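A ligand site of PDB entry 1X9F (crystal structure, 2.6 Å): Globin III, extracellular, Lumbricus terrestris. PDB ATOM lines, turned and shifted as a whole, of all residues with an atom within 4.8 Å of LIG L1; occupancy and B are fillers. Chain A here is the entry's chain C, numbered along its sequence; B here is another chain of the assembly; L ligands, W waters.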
ATOM      1  N   LEU A  43      17.051  14.459  35.013  1.00  0.00           N
ATOM      2  CA  LEU A  43      18.277  14.296  34.231  1.00  0.00           C
ATOM      3  C   LEU A  43      18.826  15.644  33.796  1.00  0.00           C
ATOM      4  O   LEU A  43      20.015  15.910  33.965  1.00  0.00           O
ATOM      5  CB  LEU A  43      18.054  13.387  33.023  1.00  0.00           C
ATOM      6  CG  LEU A  43      19.276  13.159  32.112  1.00  0.00           C
ATOM      7  CD1 LEU A  43      20.355  12.320  32.817  1.00  0.00           C
ATOM      8  CD2 LEU A  43      18.850  12.477  30.828  1.00  0.00           C
ATOM      9  N   LEU A  53      19.790  18.973  24.312  1.00  0.00           N
ATOM     10  CA  LEU A  53      19.547  17.716  23.596  1.00  0.00           C
ATOM     11  C   LEU A  53      18.067  17.477  23.329  1.00  0.00           C
ATOM     12  O   LEU A  53      17.704  16.836  22.331  1.00  0.00           O
ATOM     13  CB  LEU A  53      20.159  16.543  24.381  1.00  0.00           C
ATOM     14  CG  LEU A  53      21.656  16.654  24.681  1.00  0.00           C
ATOM     15  CD1 LEU A  53      22.055  15.758  25.837  1.00  0.00           C
ATOM     16  CD2 LEU A  53      22.468  16.319  23.451  1.00  0.00           C
ATOM     17  N   PHE A  54      17.210  18.006  24.202  1.00  0.00           N
ATOM     18  CA  PHE A  54      15.765  17.821  24.101  1.00  0.00           C
ATOM     19  C   PHE A  54      14.990  19.067  23.612  1.00  0.00           C
ATOM     20  O   PHE A  54      13.776  19.173  23.829  1.00  0.00           O
ATOM     21  CB  PHE A  54      15.209  17.314  25.446  1.00  0.00           C
ATOM     22  CG  PHE A  54      15.634  15.911  25.789  1.00  0.00           C
ATOM     23  CD1 PHE A  54      16.470  15.661  26.878  1.00  0.00           C
ATOM     24  CD2 PHE A  54      15.204  14.831  25.031  1.00  0.00           C
ATOM     25  CE1 PHE A  54      16.858  14.363  27.197  1.00  0.00           C
ATOM     26  CE2 PHE A  54      15.591  13.549  25.345  1.00  0.00           C
ATOM     27  CZ  PHE A  54      16.418  13.310  26.434  1.00  0.00           C
ATOM     28  N   ARG A  56      14.349  19.875  20.477  1.00  0.00           N
ATOM     29  CA  ARG A  56      13.481  19.402  19.407  1.00  0.00           C
ATOM     30  C   ARG A  56      12.145  18.879  19.950  1.00  0.00           C
ATOM     31  O   ARG A  56      11.131  18.908  19.251  1.00  0.00           O
ATOM     32  CB  ARG A  56      14.210  18.317  18.579  1.00  0.00           C
ATOM     33  CG  ARG A  56      13.768  18.162  17.118  1.00  0.00           C
ATOM     34  CD  ARG A  56      12.466  17.376  16.906  1.00  0.00           C
ATOM     35  NE  ARG A  56      12.599  15.920  17.026  1.00  0.00           N
ATOM     36  CZ  ARG A  56      11.569  15.076  17.182  1.00  0.00           C
ATOM     37  NH1 ARG A  56      10.325  15.539  17.264  1.00  0.00           N
ATOM     38  NH2 ARG A  56      11.782  13.768  17.274  1.00  0.00           N
ATOM     39  N   VAL A  57      12.135  18.419  21.199  1.00  0.00           N
ATOM     40  CA  VAL A  57      10.901  17.893  21.790  1.00  0.00           C
ATOM     41  C   VAL A  57      10.249  18.816  22.818  1.00  0.00           C
ATOM     42  O   VAL A  57       9.296  18.431  23.492  1.00  0.00           O
ATOM     43  CB  VAL A  57      11.061  16.460  22.366  1.00  0.00           C
ATOM     44  CG1 VAL A  57      11.205  15.446  21.242  1.00  0.00           C
ATOM     45  CG2 VAL A  57      12.223  16.375  23.347  1.00  0.00           C
ATOM     46  N   HIS A  70       7.066  12.544  23.612  1.00  0.00           N
ATOM     47  CA  HIS A  70       8.405  12.047  23.755  1.00  0.00           C
ATOM     48  C   HIS A  70       8.566  11.168  25.000  1.00  0.00           C
ATOM     49  O   HIS A  70       9.211  10.122  24.959  1.00  0.00           O
ATOM     50  CB  HIS A  70       9.360  13.208  23.816  1.00  0.00           C
ATOM     51  CG  HIS A  70      10.757  12.810  24.128  1.00  0.00           C
ATOM     52  ND1 HIS A  70      11.586  12.232  23.194  1.00  0.00           N
ATOM     53  CD2 HIS A  70      11.474  12.895  25.272  1.00  0.00           C
ATOM     54  CE1 HIS A  70      12.759  11.986  23.753  1.00  0.00           C
ATOM     55  NE2 HIS A  70      12.712  12.374  25.021  1.00  0.00           N
ATOM     56  N   ARG A  73       7.323   7.983  24.417  1.00  0.00           N
ATOM     57  CA  ARG A  73       8.231   7.315  23.503  1.00  0.00           C
ATOM     58  C   ARG A  73       9.375   6.622  24.241  1.00  0.00           C
ATOM     59  O   ARG A  73       9.618   5.433  24.007  1.00  0.00           O
ATOM     60  CB  ARG A  73       8.741   8.302  22.458  1.00  0.00           C
ATOM     61  CG  ARG A  73       8.608   7.796  21.029  1.00  0.00           C
ATOM     62  CD  ARG A  73       8.034   8.818  20.054  1.00  0.00           C
ATOM     63  NE  ARG A  73       8.734  10.088  20.151  1.00  0.00           N
ATOM     64  CZ  ARG A  73       8.169  11.281  20.005  1.00  0.00           C
ATOM     65  NH1 ARG A  73       6.867  11.398  19.756  1.00  0.00           N
ATOM     66  NH2 ARG A  73       8.916  12.374  20.121  1.00  0.00           N
ATOM     67  N   ILE A  74      10.067   7.343  25.123  1.00  0.00           N
ATOM     68  CA  ILE A  74      11.141   6.740  25.924  1.00  0.00           C
ATOM     69  C   ILE A  74      10.627   5.670  26.862  1.00  0.00           C
ATOM     70  O   ILE A  74      11.274   4.635  27.062  1.00  0.00           O
ATOM     71  CB  ILE A  74      11.909   7.791  26.764  1.00  0.00           C
ATOM     72  CG1 ILE A  74      12.894   7.060  27.695  1.00  0.00           C
ATOM     73  CG2 ILE A  74      10.941   8.661  27.578  1.00  0.00           C
ATOM     74  CD1 ILE A  74      13.649   7.943  28.717  1.00  0.00           C
ATOM     75  N   GLY A  77      10.030   2.688  25.071  1.00  0.00           N
ATOM     76  CA  GLY A  77      11.330   2.124  24.712  1.00  0.00           C
ATOM     77  C   GLY A  77      11.824   1.246  25.842  1.00  0.00           C
ATOM     78  O   GLY A  77      12.323   0.142  25.608  1.00  0.00           O
ATOM     79  N   LEU A  78      11.682   1.749  27.072  1.00  0.00           N
ATOM     80  CA  LEU A  78      12.086   1.007  28.267  1.00  0.00           C
ATOM     81  C   LEU A  78      11.136  -0.175  28.502  1.00  0.00           C
ATOM     82  O   LEU A  78      11.566  -1.255  28.904  1.00  0.00           O
ATOM     83  CB  LEU A  78      12.141   1.931  29.490  1.00  0.00           C
ATOM     84  CG  LEU A  78      12.477   1.316  30.862  1.00  0.00           C
ATOM     85  CD1 LEU A  78      13.856   0.655  30.850  1.00  0.00           C
ATOM     86  CD2 LEU A  78      12.390   2.364  31.961  1.00  0.00           C
ATOM     87  N   LEU A  98      17.741   1.097  19.201  1.00  0.00           N
ATOM     88  CA  LEU A  98      17.814   2.246  20.095  1.00  0.00           C
ATOM     89  C   LEU A  98      19.222   2.853  20.106  1.00  0.00           C
ATOM     90  O   LEU A  98      19.368   4.078  20.088  1.00  0.00           O
ATOM     91  CB  LEU A  98      17.366   1.883  21.519  1.00  0.00           C
ATOM     92  CG  LEU A  98      15.877   1.587  21.730  1.00  0.00           C
ATOM     93  CD1 LEU A  98      15.634   0.802  23.020  1.00  0.00           C
ATOM     94  CD2 LEU A  98      15.058   2.882  21.725  1.00  0.00           C
ATOM     95  N   GLN A 101      19.623   5.056  17.141  1.00  0.00           N
ATOM     96  CA  GLN A 101      18.816   6.246  17.296  1.00  0.00           C
ATOM     97  C   GLN A 101      19.473   7.321  18.189  1.00  0.00           C
ATOM     98  O   GLN A 101      19.306   8.512  17.917  1.00  0.00           O
ATOM     99  CB  GLN A 101      17.404   5.914  17.812  1.00  0.00           C
ATOM    100  CG  GLN A 101      16.543   5.127  16.803  1.00  0.00           C
ATOM    101  CD  GLN A 101      15.136   4.878  17.315  1.00  0.00           C
ATOM    102  OE1 GLN A 101      14.948   4.461  18.463  1.00  0.00           O
ATOM    103  NE2 GLN A 101      14.142   5.107  16.461  1.00  0.00           N
ATOM    104  N   HIS A 102      20.212   6.910  19.222  1.00  0.00           N
ATOM    105  CA  HIS A 102      20.892   7.903  20.074  1.00  0.00           C
ATOM    106  C   HIS A 102      22.224   8.318  19.486  1.00  0.00           C
ATOM    107  O   HIS A 102      22.676   9.446  19.685  1.00  0.00           O
ATOM    108  CB  HIS A 102      21.054   7.397  21.522  1.00  0.00           C
ATOM    109  CG  HIS A 102      19.754   7.310  22.267  1.00  0.00           C
ATOM    110  ND1 HIS A 102      18.839   6.311  22.038  1.00  0.00           N
ATOM    111  CD2 HIS A 102      19.207   8.116  23.210  1.00  0.00           C
ATOM    112  CE1 HIS A 102      17.785   6.496  22.808  1.00  0.00           C
ATOM    113  NE2 HIS A 102      17.981   7.585  23.538  1.00  0.00           N
ATOM    114  N   ARG A 105      22.338  11.425  17.482  1.00  0.00           N
ATOM    115  CA  ARG A 105      22.085  12.690  18.194  1.00  0.00           C
ATOM    116  C   ARG A 105      23.391  13.180  18.777  1.00  0.00           C
ATOM    117  O   ARG A 105      23.938  12.544  19.678  1.00  0.00           O
ATOM    118  CB  ARG A 105      21.094  12.492  19.347  1.00  0.00           C
ATOM    119  CG  ARG A 105      19.943  11.545  19.070  1.00  0.00           C
ATOM    120  CD  ARG A 105      19.048  11.989  17.938  1.00  0.00           C
ATOM    121  NE  ARG A 105      18.578  13.353  18.152  1.00  0.00           N
ATOM    122  CZ  ARG A 105      17.850  14.031  17.279  1.00  0.00           C
ATOM    123  NH1 ARG A 105      17.491  13.479  16.127  1.00  0.00           N
ATOM    124  NH2 ARG A 105      17.473  15.270  17.558  1.00  0.00           N
ATOM    125  N   VAL A 108      24.637  13.665  23.051  1.00  0.00           N
ATOM    126  CA  VAL A 108      24.236  12.546  23.888  1.00  0.00           C
ATOM    127  C   VAL A 108      25.459  11.672  24.152  1.00  0.00           C
ATOM    128  O   VAL A 108      26.089  11.202  23.208  1.00  0.00           O
ATOM    129  CB  VAL A 108      23.112  11.715  23.209  1.00  0.00           C
ATOM    130  CG1 VAL A 108      22.860  10.415  23.955  1.00  0.00           C
ATOM    131  CG2 VAL A 108      21.828  12.536  23.120  1.00  0.00           C
ATOM    132  N   GLN A 109      25.814  11.504  25.421  1.00  0.00           N
ATOM    133  CA  GLN A 109      27.026  10.772  25.749  1.00  0.00           C
ATOM    134  C   GLN A 109      26.847   9.759  26.868  1.00  0.00           C
ATOM    135  O   GLN A 109      25.895   9.853  27.650  1.00  0.00           O
ATOM    136  CB  GLN A 109      28.178  11.745  26.058  1.00  0.00           C
ATOM    137  CG  GLN A 109      27.833  12.811  27.079  1.00  0.00           C
ATOM    138  CD  GLN A 109      28.791  13.982  27.066  1.00  0.00           C
ATOM    139  OE1 GLN A 109      28.761  14.812  26.155  1.00  0.00           O
ATOM    140  NE2 GLN A 109      29.639  14.068  28.087  1.00  0.00           N
ATOM    141  N   HIS A 112      25.570  10.582  30.385  1.00  0.00           N
ATOM    142  CA  HIS A 112      24.151  10.860  30.545  1.00  0.00           C
ATOM    143  C   HIS A 112      23.372   9.595  30.911  1.00  0.00           C
ATOM    144  O   HIS A 112      22.470   9.630  31.746  1.00  0.00           O
ATOM    145  CB  HIS A 112      23.565  11.429  29.253  1.00  0.00           C
ATOM    146  CG  HIS A 112      24.157  12.729  28.808  1.00  0.00           C
ATOM    147  ND1 HIS A 112      24.072  13.153  27.497  1.00  0.00           N
ATOM    148  CD2 HIS A 112      24.805  13.707  29.480  1.00  0.00           C
ATOM    149  CE1 HIS A 112      24.645  14.344  27.384  1.00  0.00           C
ATOM    150  NE2 HIS A 112      25.101  14.702  28.572  1.00  0.00           N
ATOM    151  N   PHE A 113      23.734   8.484  30.268  1.00  0.00           N
ATOM    152  CA  PHE A 113      23.086   7.202  30.533  1.00  0.00           C
ATOM    153  C   PHE A 113      23.438   6.635  31.900  1.00  0.00           C
ATOM    154  O   PHE A 113      22.638   5.904  32.492  1.00  0.00           O
ATOM    155  CB  PHE A 113      23.405   6.197  29.432  1.00  0.00           C
ATOM    156  CG  PHE A 113      22.512   6.323  28.237  1.00  0.00           C
ATOM    157  CD1 PHE A 113      22.720   7.314  27.294  1.00  0.00           C
ATOM    158  CD2 PHE A 113      21.447   5.441  28.064  1.00  0.00           C
ATOM    159  CE1 PHE A 113      21.881   7.437  26.182  1.00  0.00           C
ATOM    160  CE2 PHE A 113      20.609   5.548  26.956  1.00  0.00           C
ATOM    161  CZ  PHE A 113      20.829   6.557  26.011  1.00  0.00           C
ATOM    162  N   PHE A 116      21.141   8.672  34.180  1.00  0.00           N
ATOM    163  CA  PHE A 116      19.786   8.184  33.993  1.00  0.00           C
ATOM    164  C   PHE A 116      19.542   6.917  34.813  1.00  0.00           C
ATOM    165  O   PHE A 116      18.536   6.820  35.524  1.00  0.00           O
ATOM    166  CB  PHE A 116      19.484   7.957  32.515  1.00  0.00           C
ATOM    167  CG  PHE A 116      18.028   7.781  32.226  1.00  0.00           C
ATOM    168  CD1 PHE A 116      17.549   6.551  31.793  1.00  0.00           C
ATOM    169  CD2 PHE A 116      17.135   8.835  32.394  1.00  0.00           C
ATOM    170  CE1 PHE A 116      16.192   6.369  31.522  1.00  0.00           C
ATOM    171  CE2 PHE A 116      15.776   8.670  32.119  1.00  0.00           C
ATOM    172  CZ  PHE A 116      15.299   7.424  31.690  1.00  0.00           C
ATOM    173  N   LEU A 120      16.823   6.500  37.591  1.00  0.00           N
ATOM    174  CA  LEU A 120      15.869   5.419  37.403  1.00  0.00           C
ATOM    175  C   LEU A 120      15.854   4.487  38.615  1.00  0.00           C
ATOM    176  O   LEU A 120      14.784   4.039  39.046  1.00  0.00           O
ATOM    177  CB  LEU A 120      16.242   4.648  36.131  1.00  0.00           C
ATOM    178  CG  LEU A 120      15.240   3.766  35.387  1.00  0.00           C
ATOM    179  CD1 LEU A 120      13.875   4.438  35.233  1.00  0.00           C
ATOM    180  CD2 LEU A 120      15.813   3.428  34.016  1.00  0.00           C
ATOM    181  N   LEU A 144      20.888  -0.065  29.493  1.00  0.00           N
ATOM    182  CA  LEU A 144      21.563   1.237  29.386  1.00  0.00           C
ATOM    183  C   LEU A 144      22.913   1.178  28.705  1.00  0.00           C
ATOM    184  O   LEU A 144      23.253   2.075  27.928  1.00  0.00           O
ATOM    185  CB  LEU A 144      21.731   1.850  30.776  1.00  0.00           C
ATOM    186  CG  LEU A 144      20.401   2.217  31.458  1.00  0.00           C
ATOM    187  CD1 LEU A 144      20.657   2.560  32.912  1.00  0.00           C
ATOM    188  CD2 LEU A 144      19.715   3.387  30.751  1.00  0.00           C
ATOM    189  N   ILE A 147      22.196   0.500  24.779  1.00  0.00           N
ATOM    190  CA  ILE A 147      21.717   1.710  24.096  1.00  0.00           C
ATOM    191  C   ILE A 147      22.830   2.749  23.950  1.00  0.00           C
ATOM    192  O   ILE A 147      22.886   3.458  22.939  1.00  0.00           O
ATOM    193  CB  ILE A 147      20.495   2.318  24.836  1.00  0.00           C
ATOM    194  CG1 ILE A 147      19.370   1.278  24.916  1.00  0.00           C
ATOM    195  CG2 ILE A 147      19.988   3.560  24.123  1.00  0.00           C
ATOM    196  CD1 ILE A 147      18.259   1.626  25.904  1.00  0.00           C
ATOM    197  N   HIS B  91       5.157  12.531  14.505  1.00  0.00           N
ATOM    198  CA  HIS B  91       6.431  11.835  14.663  1.00  0.00           C
ATOM    199  C   HIS B  91       6.461  10.596  13.779  1.00  0.00           C
ATOM    200  O   HIS B  91       7.437  10.361  13.046  1.00  0.00           O
ATOM    201  CB  HIS B  91       6.663  11.452  16.125  1.00  0.00           C
ATOM    202  CG  HIS B  91       8.028  10.896  16.394  1.00  0.00           C
ATOM    203  ND1 HIS B  91       9.132  11.692  16.571  1.00  0.00           N
ATOM    204  CD2 HIS B  91       8.452   9.614  16.544  1.00  0.00           C
ATOM    205  CE1 HIS B  91      10.189  10.931  16.795  1.00  0.00           C
ATOM    206  NE2 HIS B  91       9.805   9.669  16.791  1.00  0.00           N
ATOM    207  N   GLN B  95       8.409   9.446  10.097  1.00  0.00           N
ATOM    208  CA  GLN B  95       9.112   8.178   9.926  1.00  0.00           C
ATOM    209  C   GLN B  95       8.610   7.359   8.738  1.00  0.00           C
ATOM    210  O   GLN B  95       9.317   6.481   8.258  1.00  0.00           O
ATOM    211  CB  GLN B  95       9.063   7.344  11.201  1.00  0.00           C
ATOM    212  CG  GLN B  95       9.918   7.887  12.311  1.00  0.00           C
ATOM    213  CD  GLN B  95       9.651   7.234  13.656  1.00  0.00           C
ATOM    214  OE1 GLN B  95       8.532   6.775  13.928  1.00  0.00           O
ATOM    215  NE2 GLN B  95      10.666   7.215  14.502  1.00  0.00           N
HETATM  216  C1  LIG L   1      14.936   9.743  21.638  1.00  0.00           C
HETATM  217  C2  LIG L   1      14.501   5.593  24.204  1.00  0.00           C
HETATM  218  C3  LIG L   1      17.683   7.227  27.523  1.00  0.00           C
HETATM  219  C4  LIG L   1      18.387  11.224  24.756  1.00  0.00           C
HETATM  220  C5  LIG L   1      14.460   8.424  22.091  1.00  0.00           C
HETATM  221  C6  LIG L   1      13.464   7.733  21.406  1.00  0.00           C
HETATM  222  C7  LIG L   1      13.295   6.478  22.137  1.00  0.00           C
HETATM  223  C8  LIG L   1      14.284   6.645  23.213  1.00  0.00           C
HETATM  224  C9  LIG L   1      12.359   5.330  21.875  1.00  0.00           C
HETATM  225  C10 LIG L   1      12.704   8.180  20.181  1.00  0.00           C
HETATM  226  C11 LIG L   1      13.295   7.520  18.947  1.00  0.00           C
HETATM  227  C12 LIG L   1      12.478   7.969  17.767  1.00  0.00           C
HETATM  228  O1  LIG L   1      11.393   7.382  17.536  1.00  0.00           O
HETATM  229  O2  LIG L   1      12.902   8.912  17.070  1.00  0.00           O
HETATM  230  C13 LIG L   1      15.365   5.674  25.378  1.00  0.00           C
HETATM  231  C14 LIG L   1      15.359   4.667  26.333  1.00  0.00           C
HETATM  232  C15 LIG L   1      16.231   5.178  27.232  1.00  0.00           C
HETATM  233  C16 LIG L   1      16.710   6.393  26.794  1.00  0.00           C
HETATM  234  C17 LIG L   1      14.600   3.363  26.372  1.00  0.00           C
HETATM  235  C18 LIG L   1      16.608   4.530  28.338  1.00  0.00           C
HETATM  236  C19 LIG L   1      16.713   3.643  29.370  1.00  0.00           C
HETATM  237  C20 LIG L   1      18.158   8.536  27.034  1.00  0.00           C
HETATM  238  C21 LIG L   1      19.071   9.280  27.760  1.00  0.00           C
HETATM  239  C22 LIG L   1      19.254  10.377  26.953  1.00  0.00           C
HETATM  240  C23 LIG L   1      18.444  10.248  25.851  1.00  0.00           C
HETATM  241  C24 LIG L   1      19.732   8.962  29.072  1.00  0.00           C
HETATM  242  C25 LIG L   1      20.117  11.540  27.271  1.00  0.00           C
HETATM  243  C26 LIG L   1      21.318  11.918  26.675  1.00  0.00           C
HETATM  244  C27 LIG L   1      17.473  11.185  23.597  1.00  0.00           C
HETATM  245  C28 LIG L   1      17.407  12.245  22.701  1.00  0.00           C
HETATM  246  C29 LIG L   1      16.449  11.872  21.787  1.00  0.00           C
HETATM  247  C30 LIG L   1      15.991  10.540  22.276  1.00  0.00           C
HETATM  248  C31 LIG L   1      18.226  13.515  22.720  1.00  0.00           C
HETATM  249  C32 LIG L   1      15.958  12.628  20.583  1.00  0.00           C
HETATM  250  C33 LIG L   1      14.842  13.562  21.056  1.00  0.00           C
HETATM  251  C34 LIG L   1      14.288  14.217  19.829  1.00  0.00           C
HETATM  252  O3  LIG L   1      14.777  15.289  19.438  1.00  0.00           O
HETATM  253  O4  LIG L   1      13.336  13.630  19.253  1.00  0.00           O
HETATM  254  N1  LIG L   1      15.005   7.788  23.167  1.00  0.00           N
HETATM  255  N2  LIG L   1      16.161   6.761  25.612  1.00  0.00           N
HETATM  256  N3  LIG L   1      17.760   9.079  25.858  1.00  0.00           N
HETATM  257  N4  LIG L   1      16.638  10.140  23.397  1.00  0.00           N
HETATM  258 FE1  LIG L   1      16.415   8.431  24.484  1.00  0.00          FE
HETATM  259  C1  LG2 L   2      14.741   9.595  25.638  1.00  0.00           C
HETATM  260  O1  LG2 L   2      14.268  10.183  26.594  1.00  0.00           O
HETATM  261  C1  LG3 L   3       8.712   1.611  11.007  1.00  0.00           C
HETATM  262  C2  LG3 L   3       4.545   2.554  13.384  1.00  0.00           C
HETATM  263  C3  LG3 L   3       1.962   1.057   9.510  1.00  0.00           C
HETATM  264  C4  LG3 L   3       6.135   0.357   7.033  1.00  0.00           C
HETATM  265  C5  LG3 L   3       7.750   1.939  12.077  1.00  0.00           C
HETATM  266  C6  LG3 L   3       8.217   2.306  13.337  1.00  0.00           C
HETATM  267  C7  LG3 L   3       7.000   2.590  14.102  1.00  0.00           C
HETATM  268  C8  LG3 L   3       5.961   2.351  13.084  1.00  0.00           C
HETATM  269  C9  LG3 L   3       6.875   3.018  15.538  1.00  0.00           C
HETATM  270  C10 LG3 L   3       9.639   2.334  13.842  1.00  0.00           C
HETATM  271  C11 LG3 L   3      10.302   3.690  13.714  1.00  0.00           C
HETATM  272  C12 LG3 L   3      11.728   3.491  14.175  1.00  0.00           C
HETATM  273  O1  LG3 L   3      11.971   3.416  15.397  1.00  0.00           O
HETATM  274  O2  LG3 L   3      12.616   3.383  13.297  1.00  0.00           O
HETATM  275  C13 LG3 L   3       3.445   2.199  12.488  1.00  0.00           C
HETATM  276  C14 LG3 L   3       2.144   2.294  12.933  1.00  0.00           C
HETATM  277  C15 LG3 L   3       1.459   1.888  11.834  1.00  0.00           C
HETATM  278  C16 LG3 L   3       2.332   1.564  10.829  1.00  0.00           C
HETATM  279  C17 LG3 L   3       1.614   2.736  14.272  1.00  0.00           C
HETATM  280  C18 LG3 L   3       0.123   1.830  11.881  1.00  0.00           C
HETATM  281  C19 LG3 L   3      -1.185   1.838  12.031  1.00  0.00           C
HETATM  282  C20 LG3 L   3       2.932   0.674   8.477  1.00  0.00           C
HETATM  283  C21 LG3 L   3       2.483   0.135   7.285  1.00  0.00           C
HETATM  284  C22 LG3 L   3       3.660  -0.064   6.581  1.00  0.00           C
HETATM  285  C23 LG3 L   3       4.705   0.355   7.400  1.00  0.00           C
HETATM  286  C24 LG3 L   3       1.051  -0.121   6.893  1.00  0.00           C
HETATM  287  C25 LG3 L   3       3.727  -0.624   5.208  1.00  0.00           C
HETATM  288  C26 LG3 L   3       3.190  -1.834   4.973  1.00  0.00           C
HETATM  289  C27 LG3 L   3       7.262   0.661   7.933  1.00  0.00           C
HETATM  290  C28 LG3 L   3       8.589   0.463   7.541  1.00  0.00           C
HETATM  291  C29 LG3 L   3       9.348   0.801   8.631  1.00  0.00           C
HETATM  292  C30 LG3 L   3       8.351   1.199   9.639  1.00  0.00           C
HETATM  293  C31 LG3 L   3       9.074  -0.013   6.198  1.00  0.00           C
HETATM  294  C32 LG3 L   3      10.852   0.808   8.770  1.00  0.00           C
HETATM  295  C33 LG3 L   3      11.403  -0.608   8.895  1.00  0.00           C
HETATM  296  C34 LG3 L   3      12.893  -0.477   9.073  1.00  0.00           C
HETATM  297  O3  LG3 L   3      13.340   0.104  10.087  1.00  0.00           O
HETATM  298  O4  LG3 L   3      13.630  -0.955   8.200  1.00  0.00           O
HETATM  299  N1  LG3 L   3       6.401   1.994  11.858  1.00  0.00           N
HETATM  300  N2  LG3 L   3       3.614   1.761  11.220  1.00  0.00           N
HETATM  301  N3  LG3 L   3       4.275   0.853   8.588  1.00  0.00           N
HETATM  302  N4  LG3 L   3       7.073   1.093   9.204  1.00  0.00           N
HETATM  303 FE1  LG3 L   3       5.345   1.499  10.189  1.00  0.00          FE
HETATM  304  O   HOH W   1      10.480   5.263  19.083  1.00  0.00           O
HETATM  305  O   HOH W   2      11.769  11.460  20.425  1.00  0.00           O
HETATM  306  O   HOH W   3       8.615   6.032  16.782  1.00  0.00           O
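NH2 of Arg 105 lies within salt-bridge range of O3 of LIG L1 (3.3 Å). The side-chain amide nitrogen (NE2) of Gln 101 lies within hydrogen-bond range of an oxygen (O1) of LG3 L3 (3.0 Å). O1 of LIG L1 is in hydrogen-bond range of NE2 of Gln 95 of chain B (3.1 Å). An oxygen (O1) of LIG L1 is in hydrogen-bond range of a ring nitrogen (NE2) of His 91 of chain B. NE2 of His 102 binds FE1 of LIG L1 (2.0 Å). A ring nitrogen (NE2) of His 70 sits at hydrogen-bond distance from an oxygen (O1) of LG2 L2 (3.1 Å). An oxygen (O4) of LIG L1 lies within salt-bridge range of the guanidinium group of Arg 56, at 2.5 Å.
A ring nitrogen (ND1) of His 102 lies within hydrogen-bond range of the backbone carbonyl oxygen of Leu 98 (3.0 Å). NE2 of His 91 of chain B lies within hydrogen-bond range of NE2 of Gln 95 of chain B (3.5 Å). The guanidinium group (NH2) of Arg 56 sits close to a ring nitrogen (ND1) of His 91 of chain B (3.4 Å). A ring nitrogen (ND1) of His 112 lies within hydrogen-bond range of the backbone NH of Gln 109 (3.2 Å).
CD2 of Leu 43 touches C25 of LIG L1, at 3.9 Å. Leu 53 touches LIG L1. Phe 54 touches LIG L1. Val 57 touches LIG L1. His 70 touches LIG L1. O of Arg 73 touches C9 of LIG L1 (3.5 Å). Ile 74 touches LIG L1. Gly 77 touches LIG L1 (C to C17, 3.5 Å). Leu 78 touches LIG L1 (N to C17, 3.4 Å). CD2 of Leu 98 touches C9 of LIG L1 (3.6 Å). Gln 101 touches LIG L1. Val 108 touches LIG L1. ND1 of His 112 touches C26 of LIG L1, 3.1 Å away. Phe 113 touches LIG L1. Phe 116 touches LIG L1. CD2 of Leu 144 touches C19 of LIG L1, at 3.3 Å. Hydrophobic or aromatic side chains that line LIG L1: Leu 43, Leu 53, Phe 54, Val 57, His 70, Ile 74, Leu 98, His 102, Val 108, His 112, Phe 113, Phe 116, Leu 144 and His 91 of chain B. Of the 24 residues printed, 21 come within 4 Å of LIG L1. The nearest printed residue that does not touch LIG L1 is Ile 147 (4.1 Å).
Water W2 lies within hydrogen-bond range of a ring nitrogen (ND1) of His 70, an oxygen (O4) of LIG L1 and the guanidinium group (NH2) of Arg 73. Water W3 bridges the side-chain amide oxygen of Gln 95 of chain B and an oxygen (O1) of LIG L1.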
